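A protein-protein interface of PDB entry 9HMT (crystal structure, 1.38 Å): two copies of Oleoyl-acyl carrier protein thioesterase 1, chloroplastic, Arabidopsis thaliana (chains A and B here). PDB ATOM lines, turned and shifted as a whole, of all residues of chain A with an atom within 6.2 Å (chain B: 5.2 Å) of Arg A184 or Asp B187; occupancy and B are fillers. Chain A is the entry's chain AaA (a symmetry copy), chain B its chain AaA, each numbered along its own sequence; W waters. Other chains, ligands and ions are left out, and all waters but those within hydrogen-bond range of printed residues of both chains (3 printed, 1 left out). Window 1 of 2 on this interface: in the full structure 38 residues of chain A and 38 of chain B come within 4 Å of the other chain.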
ATOM      1  N   LYS A 182     -25.609   0.852 -22.743  1.00  0.00           N
ATOM      2  CA  LYS A 182     -25.494   1.359 -24.118  1.00  0.00           C
ATOM      3  C   LYS A 182     -24.249   0.770 -24.756  1.00  0.00           C
ATOM      4  O   LYS A 182     -23.218   0.589 -24.110  1.00  0.00           O
ATOM      5  CB  LYS A 182     -25.533   2.886 -24.158  1.00  0.00           C
ATOM      6  CG  LYS A 182     -24.452   3.613 -23.393  1.00  0.00           C
ATOM      7  CD  LYS A 182     -24.780   5.089 -23.287  1.00  0.00           C
ATOM      8  CE  LYS A 182     -23.619   5.900 -22.753  1.00  0.00           C
ATOM      9  NZ  LYS A 182     -23.958   7.345 -22.672  1.00  0.00           N
ATOM     10  N   PRO A 183     -24.337   0.448 -26.045  1.00  0.00           N
ATOM     11  CA  PRO A 183     -23.184  -0.102 -26.742  1.00  0.00           C
ATOM     12  C   PRO A 183     -22.139   0.990 -27.004  1.00  0.00           C
ATOM     13  O   PRO A 183     -22.484   2.133 -27.234  1.00  0.00           O
ATOM     14  CB  PRO A 183     -23.773  -0.622 -28.051  1.00  0.00           C
ATOM     15  CG  PRO A 183     -24.948   0.285 -28.302  1.00  0.00           C
ATOM     16  CD  PRO A 183     -25.505   0.576 -26.928  1.00  0.00           C
ATOM     17  N   ARG A 184     -20.874   0.608 -26.943  1.00  0.00           N
ATOM     18  CA  ARG A 184     -19.779   1.475 -27.411  1.00  0.00           C
ATOM     19  C   ARG A 184     -19.286   0.863 -28.722  1.00  0.00           C
ATOM     20  O   ARG A 184     -19.804  -0.185 -29.149  1.00  0.00           O
ATOM     21  CB  ARG A 184     -18.718   1.683 -26.329  1.00  0.00           C
ATOM     22  CG  ARG A 184     -18.052   0.430 -25.796  1.00  0.00           C
ATOM     23  CD  ARG A 184     -17.124   0.816 -24.662  1.00  0.00           C
ATOM     24  NE  ARG A 184     -16.413  -0.305 -24.062  1.00  0.00           N
ATOM     25  CZ  ARG A 184     -15.241  -0.791 -24.475  1.00  0.00           C
ATOM     26  NH1 ARG A 184     -14.627  -0.297 -25.544  1.00  0.00           N
ATOM     27  NH2 ARG A 184     -14.692  -1.797 -23.811  1.00  0.00           N
ATOM     28  N   ARG A 185     -18.377   1.539 -29.400  1.00  0.00           N
ATOM     29  CA  ARG A 185     -18.008   1.099 -30.762  1.00  0.00           C
ATOM     30  C   ARG A 185     -17.450  -0.325 -30.746  1.00  0.00           C
ATOM     31  O   ARG A 185     -17.711  -1.051 -31.711  1.00  0.00           O
ATOM     32  CB  ARG A 185     -17.037   2.070 -31.431  1.00  0.00           C
ATOM     33  CG  ARG A 185     -17.699   3.384 -31.810  1.00  0.00           C
ATOM     34  CD  ARG A 185     -16.824   4.182 -32.750  1.00  0.00           C
ATOM     35  NE  ARG A 185     -17.423   5.496 -32.798  1.00  0.00           N
ATOM     36  CZ  ARG A 185     -16.939   6.588 -32.214  1.00  0.00           C
ATOM     37  NH1 ARG A 185     -15.778   6.560 -31.582  1.00  0.00           N
ATOM     38  NH2 ARG A 185     -17.609   7.719 -32.316  1.00  0.00           N
ATOM     39  N   ALA A 186     -16.788  -0.759 -29.674  1.00  0.00           N
ATOM     40  CA  ALA A 186     -16.215  -2.126 -29.613  1.00  0.00           C
ATOM     41  C   ALA A 186     -17.340  -3.165 -29.667  1.00  0.00           C
ATOM     42  O   ALA A 186     -17.059  -4.306 -30.043  1.00  0.00           O
ATOM     43  CB  ALA A 186     -15.370  -2.306 -28.379  1.00  0.00           C
ATOM     44  N   ASP A 187     -18.566  -2.784 -29.292  1.00  0.00           N
ATOM     45  CA  ASP A 187     -19.734  -3.698 -29.261  1.00  0.00           C
ATOM     46  C   ASP A 187     -20.307  -3.885 -30.662  1.00  0.00           C
ATOM     47  O   ASP A 187     -21.228  -4.730 -30.804  1.00  0.00           O
ATOM     48  CB  ASP A 187     -20.813  -3.159 -28.325  1.00  0.00           C
ATOM     49  CG  ASP A 187     -20.386  -3.166 -26.874  1.00  0.00           C
ATOM     50  OD1 ASP A 187     -19.868  -4.216 -26.442  1.00  0.00           O
ATOM     51  OD2 ASP A 187     -20.531  -2.128 -26.184  1.00  0.00           O
ATOM     52  N   LEU A 188     -19.886  -3.074 -31.629  1.00  0.00           N
ATOM     53  CA  LEU A 188     -20.457  -3.106 -32.992  1.00  0.00           C
ATOM     54  C   LEU A 188     -19.622  -4.030 -33.859  1.00  0.00           C
ATOM     55  O   LEU A 188     -18.394  -4.130 -33.656  1.00  0.00           O
ATOM     56  CB  LEU A 188     -20.494  -1.712 -33.606  1.00  0.00           C
ATOM     57  CG  LEU A 188     -21.195  -0.643 -32.776  1.00  0.00           C
ATOM     58  CD1 LEU A 188     -21.129   0.694 -33.489  1.00  0.00           C
ATOM     59  CD2 LEU A 188     -22.640  -1.019 -32.476  1.00  0.00           C
ATOM     60  N   TRP A 202     -25.131  -8.203 -21.765  1.00  0.00           N
ATOM     61  CA  TRP A 202     -26.205  -7.359 -21.172  1.00  0.00           C
ATOM     62  C   TRP A 202     -27.189  -8.182 -20.333  1.00  0.00           C
ATOM     63  O   TRP A 202     -27.560  -7.718 -19.228  1.00  0.00           O
ATOM     64  CB  TRP A 202     -26.924  -6.581 -22.264  1.00  0.00           C
ATOM     65  CG  TRP A 202     -26.130  -5.441 -22.820  1.00  0.00           C
ATOM     66  CD1 TRP A 202     -25.091  -4.784 -22.226  1.00  0.00           C
ATOM     67  CD2 TRP A 202     -26.359  -4.788 -24.074  1.00  0.00           C
ATOM     68  NE1 TRP A 202     -24.641  -3.780 -23.045  1.00  0.00           N
ATOM     69  CE2 TRP A 202     -25.396  -3.763 -24.178  1.00  0.00           C
ATOM     70  CE3 TRP A 202     -27.249  -5.005 -25.122  1.00  0.00           C
ATOM     71  CZ2 TRP A 202     -25.354  -2.908 -25.282  1.00  0.00           C
ATOM     72  CZ3 TRP A 202     -27.185  -4.178 -26.225  1.00  0.00           C
ATOM     73  CH2 TRP A 202     -26.250  -3.146 -26.292  1.00  0.00           C
ATOM     74  N   GLU B  31      -8.586  -0.972 -30.491  1.00  0.00           N
ATOM     75  CA  GLU B  31      -8.816  -1.737 -29.246  1.00  0.00           C
ATOM     76  C   GLU B  31      -8.340  -3.178 -29.460  1.00  0.00           C
ATOM     77  O   GLU B  31      -7.710  -3.740 -28.554  1.00  0.00           O
ATOM     78  CB  GLU B  31     -10.289  -1.693 -28.860  1.00  0.00           C
ATOM     79  CG  GLU B  31     -10.782  -0.304 -28.501  1.00  0.00           C
ATOM     80  CD  GLU B  31     -11.553   0.437 -29.584  1.00  0.00           C
ATOM     81  OE1 GLU B  31     -11.173   0.388 -30.770  1.00  0.00           O
ATOM     82  OE2 GLU B  31     -12.552   1.086 -29.219  1.00  0.00           O
ATOM     83  N   LYS B 182     -19.989   3.221 -18.255  1.00  0.00           N
ATOM     84  CA  LYS B 182     -19.759   2.330 -17.109  1.00  0.00           C
ATOM     85  C   LYS B 182     -19.272   0.987 -17.621  1.00  0.00           C
ATOM     86  O   LYS B 182     -19.703   0.500 -18.665  1.00  0.00           O
ATOM     87  CB  LYS B 182     -20.998   2.227 -16.220  1.00  0.00           C
ATOM     88  CG  LYS B 182     -22.257   1.697 -16.867  1.00  0.00           C
ATOM     89  CD  LYS B 182     -23.451   1.919 -15.962  1.00  0.00           C
ATOM     90  CE  LYS B 182     -24.685   1.189 -16.448  1.00  0.00           C
ATOM     91  NZ  LYS B 182     -25.839   1.409 -15.538  1.00  0.00           N
ATOM     92  N   PRO B 183     -18.344   0.373 -16.889  1.00  0.00           N
ATOM     93  CA  PRO B 183     -17.835  -0.929 -17.295  1.00  0.00           C
ATOM     94  C   PRO B 183     -18.879  -2.022 -17.033  1.00  0.00           C
ATOM     95  O   PRO B 183     -19.626  -1.947 -16.078  1.00  0.00           O
ATOM     96  CB  PRO B 183     -16.606  -1.123 -16.411  1.00  0.00           C
ATOM     97  CG  PRO B 183     -16.935  -0.352 -15.161  1.00  0.00           C
ATOM     98  CD  PRO B 183     -17.716   0.847 -15.647  1.00  0.00           C
ATOM     99  N   ARG B 184     -18.914  -3.011 -17.911  1.00  0.00           N
ATOM    100  CA  ARG B 184     -19.681  -4.244 -17.660  1.00  0.00           C
ATOM    101  C   ARG B 184     -18.649  -5.331 -17.362  1.00  0.00           C
ATOM    102  O   ARG B 184     -17.436  -5.059 -17.397  1.00  0.00           O
ATOM    103  CB  ARG B 184     -20.660  -4.544 -18.798  1.00  0.00           C
ATOM    104  CG  ARG B 184     -20.051  -4.711 -20.176  1.00  0.00           C
ATOM    105  CD  ARG B 184     -21.169  -4.885 -21.184  1.00  0.00           C
ATOM    106  NE  ARG B 184     -20.716  -5.062 -22.557  1.00  0.00           N
ATOM    107  CZ  ARG B 184     -20.406  -6.227 -23.127  1.00  0.00           C
ATOM    108  NH1 ARG B 184     -20.444  -7.364 -22.441  1.00  0.00           N
ATOM    109  NH2 ARG B 184     -20.039  -6.243 -24.399  1.00  0.00           N
ATOM    110  N   ARG B 185     -19.107  -6.510 -16.983  1.00  0.00           N
ATOM    111  CA  ARG B 185     -18.162  -7.536 -16.494  1.00  0.00           C
ATOM    112  C   ARG B 185     -17.128  -7.885 -17.566  1.00  0.00           C
ATOM    113  O   ARG B 185     -15.981  -8.147 -17.189  1.00  0.00           O
ATOM    114  CB  ARG B 185     -18.884  -8.783 -15.989  1.00  0.00           C
ATOM    115  CG  ARG B 185     -19.620  -8.539 -14.683  1.00  0.00           C
ATOM    116  CD  ARG B 185     -20.041  -9.843 -14.044  1.00  0.00           C
ATOM    117  NE  ARG B 185     -20.956  -9.469 -12.991  1.00  0.00           N
ATOM    118  CZ  ARG B 185     -22.276  -9.630 -13.020  1.00  0.00           C
ATOM    119  NH1 ARG B 185     -22.861 -10.244 -14.035  1.00  0.00           N
ATOM    120  NH2 ARG B 185     -22.995  -9.213 -11.997  1.00  0.00           N
ATOM    121  N   ALA B 186     -17.467  -7.811 -18.852  1.00  0.00           N
ATOM    122  CA  ALA B 186     -16.507  -8.153 -19.932  1.00  0.00           C
ATOM    123  C   ALA B 186     -15.330  -7.171 -19.911  1.00  0.00           C
ATOM    124  O   ALA B 186     -14.268  -7.528 -20.427  1.00  0.00           O
ATOM    125  CB  ALA B 186     -17.183  -8.161 -21.278  1.00  0.00           C
ATOM    126  N   ASP B 187     -15.521  -5.974 -19.347  1.00  0.00           N
ATOM    127  CA  ASP B 187     -14.479  -4.919 -19.294  1.00  0.00           C
ATOM    128  C   ASP B 187     -13.484  -5.202 -18.172  1.00  0.00           C
ATOM    129  O   ASP B 187     -12.478  -4.452 -18.087  1.00  0.00           O
ATOM    130  CB  ASP B 187     -15.115  -3.546 -19.091  1.00  0.00           C
ATOM    131  CG  ASP B 187     -15.936  -3.100 -20.280  1.00  0.00           C
ATOM    132  OD1 ASP B 187     -15.409  -3.215 -21.405  1.00  0.00           O
ATOM    133  OD2 ASP B 187     -17.103  -2.676 -20.100  1.00  0.00           O
ATOM    134  N   LEU B 188     -13.787  -6.145 -17.283  1.00  0.00           N
ATOM    135  CA  LEU B 188     -12.941  -6.419 -16.104  1.00  0.00           C
ATOM    136  C   LEU B 188     -11.956  -7.523 -16.444  1.00  0.00           C
ATOM    137  O   LEU B 188     -12.286  -8.425 -17.243  1.00  0.00           O
ATOM    138  CB  LEU B 188     -13.786  -6.831 -14.904  1.00  0.00           C
ATOM    139  CG  LEU B 188     -14.906  -5.870 -14.525  1.00  0.00           C
ATOM    140  CD1 LEU B 188     -15.681  -6.416 -13.342  1.00  0.00           C
ATOM    141  CD2 LEU B 188     -14.374  -4.476 -14.219  1.00  0.00           C
ATOM    142  N   ASP B 189     -10.791  -7.446 -15.830  1.00  0.00           N
ATOM    143  CA  ASP B 189      -9.740  -8.469 -16.002  1.00  0.00           C
ATOM    144  C   ASP B 189      -9.888  -9.554 -14.938  1.00  0.00           C
ATOM    145  O   ASP B 189     -10.858  -9.540 -14.160  1.00  0.00           O
ATOM    146  CB  ASP B 189      -8.374  -7.799 -15.995  1.00  0.00           C
ATOM    147  CG  ASP B 189      -7.952  -7.234 -14.652  1.00  0.00           C
ATOM    148  OD1 ASP B 189      -8.569  -7.575 -13.625  1.00  0.00           O
ATOM    149  OD2 ASP B 189      -6.986  -6.453 -14.658  1.00  0.00           O
ATOM    150  N   HIS B 193     -10.415  -5.853 -12.025  1.00  0.00           N
ATOM    151  CA  HIS B 193     -10.044  -4.455 -12.347  1.00  0.00           C
ATOM    152  C   HIS B 193     -10.439  -4.139 -13.789  1.00  0.00           C
ATOM    153  O   HIS B 193     -10.377  -5.048 -14.641  1.00  0.00           O
ATOM    154  CB  HIS B 193      -8.536  -4.236 -12.198  1.00  0.00           C
ATOM    155  CG  HIS B 193      -8.058  -4.222 -10.788  1.00  0.00           C
ATOM    156  ND1 HIS B 193      -7.719  -3.047 -10.139  1.00  0.00           N
ATOM    157  CD2 HIS B 193      -7.842  -5.223  -9.911  1.00  0.00           C
ATOM    158  CE1 HIS B 193      -7.332  -3.330  -8.910  1.00  0.00           C
ATOM    159  NE2 HIS B 193      -7.405  -4.661  -8.743  1.00  0.00           N
ATOM    160  N   VAL B 194     -10.777  -2.898 -14.067  1.00  0.00           N
ATOM    161  CA  VAL B 194     -11.086  -2.490 -15.461  1.00  0.00           C
ATOM    162  C   VAL B 194      -9.831  -2.712 -16.317  1.00  0.00           C
ATOM    163  O   VAL B 194      -8.721  -2.309 -15.937  1.00  0.00           O
ATOM    164  CB  VAL B 194     -11.586  -1.046 -15.508  1.00  0.00           C
ATOM    165  CG1 VAL B 194     -11.763  -0.589 -16.940  1.00  0.00           C
ATOM    166  CG2 VAL B 194     -12.899  -0.910 -14.753  1.00  0.00           C
ATOM    167  N   ASN B 195     -10.002  -3.417 -17.429  1.00  0.00           N
ATOM    168  CA  ASN B 195      -8.891  -3.732 -18.361  1.00  0.00           C
ATOM    169  C   ASN B 195      -8.372  -2.420 -18.935  1.00  0.00           C
ATOM    170  O   ASN B 195      -9.203  -1.548 -19.275  1.00  0.00           O
ATOM    171  CB  ASN B 195      -9.369  -4.700 -19.443  1.00  0.00           C
ATOM    172  CG  ASN B 195      -8.267  -5.156 -20.376  1.00  0.00           C
ATOM    173  OD1 ASN B 195      -7.574  -4.351 -20.990  1.00  0.00           O
ATOM    174  ND2 ASN B 195      -8.089  -6.462 -20.488  1.00  0.00           N
ATOM    175  N   THR B 198     -10.033  -0.937 -22.067  1.00  0.00           N
ATOM    176  CA  THR B 198     -11.351  -0.287 -21.898  1.00  0.00           C
ATOM    177  C   THR B 198     -11.152   1.240 -21.901  1.00  0.00           C
ATOM    178  O   THR B 198     -11.985   1.943 -22.473  1.00  0.00           O
ATOM    179  CB  THR B 198     -12.043  -0.768 -20.620  1.00  0.00           C
ATOM    180  OG1 THR B 198     -12.197  -2.184 -20.710  1.00  0.00           O
ATOM    181  CG2 THR B 198     -13.399  -0.119 -20.442  1.00  0.00           C
ATOM    182  N   GLY B 201     -11.024   2.535 -25.406  1.00  0.00           N
ATOM    183  CA  GLY B 201     -12.377   2.612 -25.966  1.00  0.00           C
ATOM    184  C   GLY B 201     -13.133   3.816 -25.439  1.00  0.00           C
ATOM    185  O   GLY B 201     -13.805   4.509 -26.191  1.00  0.00           O
ATOM    186  N   TRP B 202     -13.071   4.032 -24.142  1.00  0.00           N
ATOM    187  CA  TRP B 202     -13.793   5.189 -23.543  1.00  0.00           C
ATOM    188  C   TRP B 202     -13.273   6.531 -24.073  1.00  0.00           C
ATOM    189  O   TRP B 202     -14.111   7.414 -24.376  1.00  0.00           O
ATOM    190  CB  TRP B 202     -13.715   5.127 -22.025  1.00  0.00           C
ATOM    191  CG  TRP B 202     -14.590   4.076 -21.415  1.00  0.00           C
ATOM    192  CD1 TRP B 202     -15.694   3.492 -21.966  1.00  0.00           C
ATOM    193  CD2 TRP B 202     -14.454   3.527 -20.100  1.00  0.00           C
ATOM    194  NE1 TRP B 202     -16.238   2.593 -21.085  1.00  0.00           N
ATOM    195  CE2 TRP B 202     -15.499   2.593 -19.941  1.00  0.00           C
ATOM    196  CE3 TRP B 202     -13.528   3.705 -19.076  1.00  0.00           C
ATOM    197  CZ2 TRP B 202     -15.674   1.886 -18.749  1.00  0.00           C
ATOM    198  CZ3 TRP B 202     -13.686   2.982 -17.911  1.00  0.00           C
ATOM    199  CH2 TRP B 202     -14.748   2.091 -17.759  1.00  0.00           C
ATOM    200  N   GLU B 205     -14.777   7.100 -27.528  1.00  0.00           N
ATOM    201  CA  GLU B 205     -16.253   7.221 -27.583  1.00  0.00           C
ATOM    202  C   GLU B 205     -16.682   8.670 -27.812  1.00  0.00           C
ATOM    203  O   GLU B 205     -17.777   8.883 -28.380  1.00  0.00           O
ATOM    204  CB  GLU B 205     -16.884   6.737 -26.288  1.00  0.00           C
ATOM    205  CG  GLU B 205     -17.249   5.268 -26.296  1.00  0.00           C
ATOM    206  CD  GLU B 205     -18.133   4.807 -27.449  1.00  0.00           C
ATOM    207  OE1 GLU B 205     -17.598   4.179 -28.374  1.00  0.00           O
ATOM    208  OE2 GLU B 205     -19.352   5.033 -27.414  1.00  0.00           O
HETATM  209  O   HOH W   1     -20.314  -2.470 -23.557  1.00  0.00           O
HETATM  210  O   HOH W   2     -18.174  -1.382 -22.160  1.00  0.00           O
HETATM  211  O   HOH W   3     -21.169   4.258 -25.377  1.00  0.00           O
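The backbone NH (N) of Arg B184 is in hydrogen-bond range of the side-chain carboxylate (OD2) of Asp B187.
The backbone NH (N) of Asn B195 sits at hydrogen-bond distance from the backbone carbonyl oxygen (O) of Asp B187 (2.8 Å).
The side-chain carboxylate of Asp B187 lies within hydrogen-bond range of the side-chain hydroxyl of Thr B198, at 3.4 Å.
O of Asn B195 sits close to OG1 of Thr B198.
The side-chain carboxylate (OD2) of Asp A187 sits at hydrogen-bond distance from the backbone NH (N) of Arg A184 (2.9 Å).
Arg A184 touches Thr B198 (NH2 to CG2, 3.98 Å).
NH1 of Arg A184 touches CA of Gly B201, at 3.7 Å.
Arg A184 touches Glu B205 (CB to CD, 3.4 Å).
Of the 16 printed residues of chain B, 5 touch a printed residue of chain A.
Printed residues of chain B that touch a printed residue of chain A: Arg B184, Asp B187, Thr B198, Gly B201 and Glu B205.
Along chain B the printed residues that touch a printed residue of chain A span positions 184 to 205.
Of the 8 printed residues of chain A, 3 touch a printed residue of chain B.
Printed residues of chain A that touch a printed residue of chain B: Arg A184, Arg A185 and Asp A187.
Among the printed residues, 6 pairs touch across the chains.
Among the printed residues, Asp or Glu carboxylates within 4 Å of a Lys or Arg side-chain nitrogen of the other chain: Arg A184 with Asp B187 and Asp A187 with Arg B184.
Printed residues of chain B within 4 Å of Arg A184: Asp B187, Thr B198, Gly B201 and Glu B205.
Of the printed residues of chain A, Arg B184 touches Asp A187.
Of the printed residues of chain A, Thr B198 touches Arg A184.
Of the printed residues of chain B, Arg A185 touches Glu B205.
Of the printed residues of chain B, Asp A187 touches Arg B184 (2.9 Å).
Printed residues of chain A within 4 Å of Gly B201: Arg A184.
Pro B183 touches none of the printed residues of chain A.
Ala B186 touches none of the printed residues of chain A.
The nearest printed residue of chain B that does not touch Arg A184 is Trp B202 (4.1 Å).
The nearest printed residue of chain A that does not touch Asp B187 is Asp A187 (6.8 Å).
Water W2 lies within hydrogen-bond range of OD2 of Asp B187 (2.7 Å) and NE of Arg A184 (2.8 Å).
Water W1 lies within hydrogen-bond range of the side-chain carboxylate of Asp A187 and the guanidinium group of Arg B184.
Water W3 lies within hydrogen-bond range of OE2 of Glu B205 (2.8 Å) and O of Pro A183 (3.1 Å).
Arg A184 touches Asp B187, and with the chains exchanged Asp A187 touches Arg B184.
OD1 of Asp A187 is in salt-bridge range of NH2 of Arg B184, at 2.9 Å.
NH2 of Arg A184 is in salt-bridge range of OD1 of Asp B187 (2.9 Å).
The backbone NH (N) of Arg A185 sits at hydrogen-bond distance from the side-chain carboxylate (OE1) of Glu B205 (2.9 Å).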
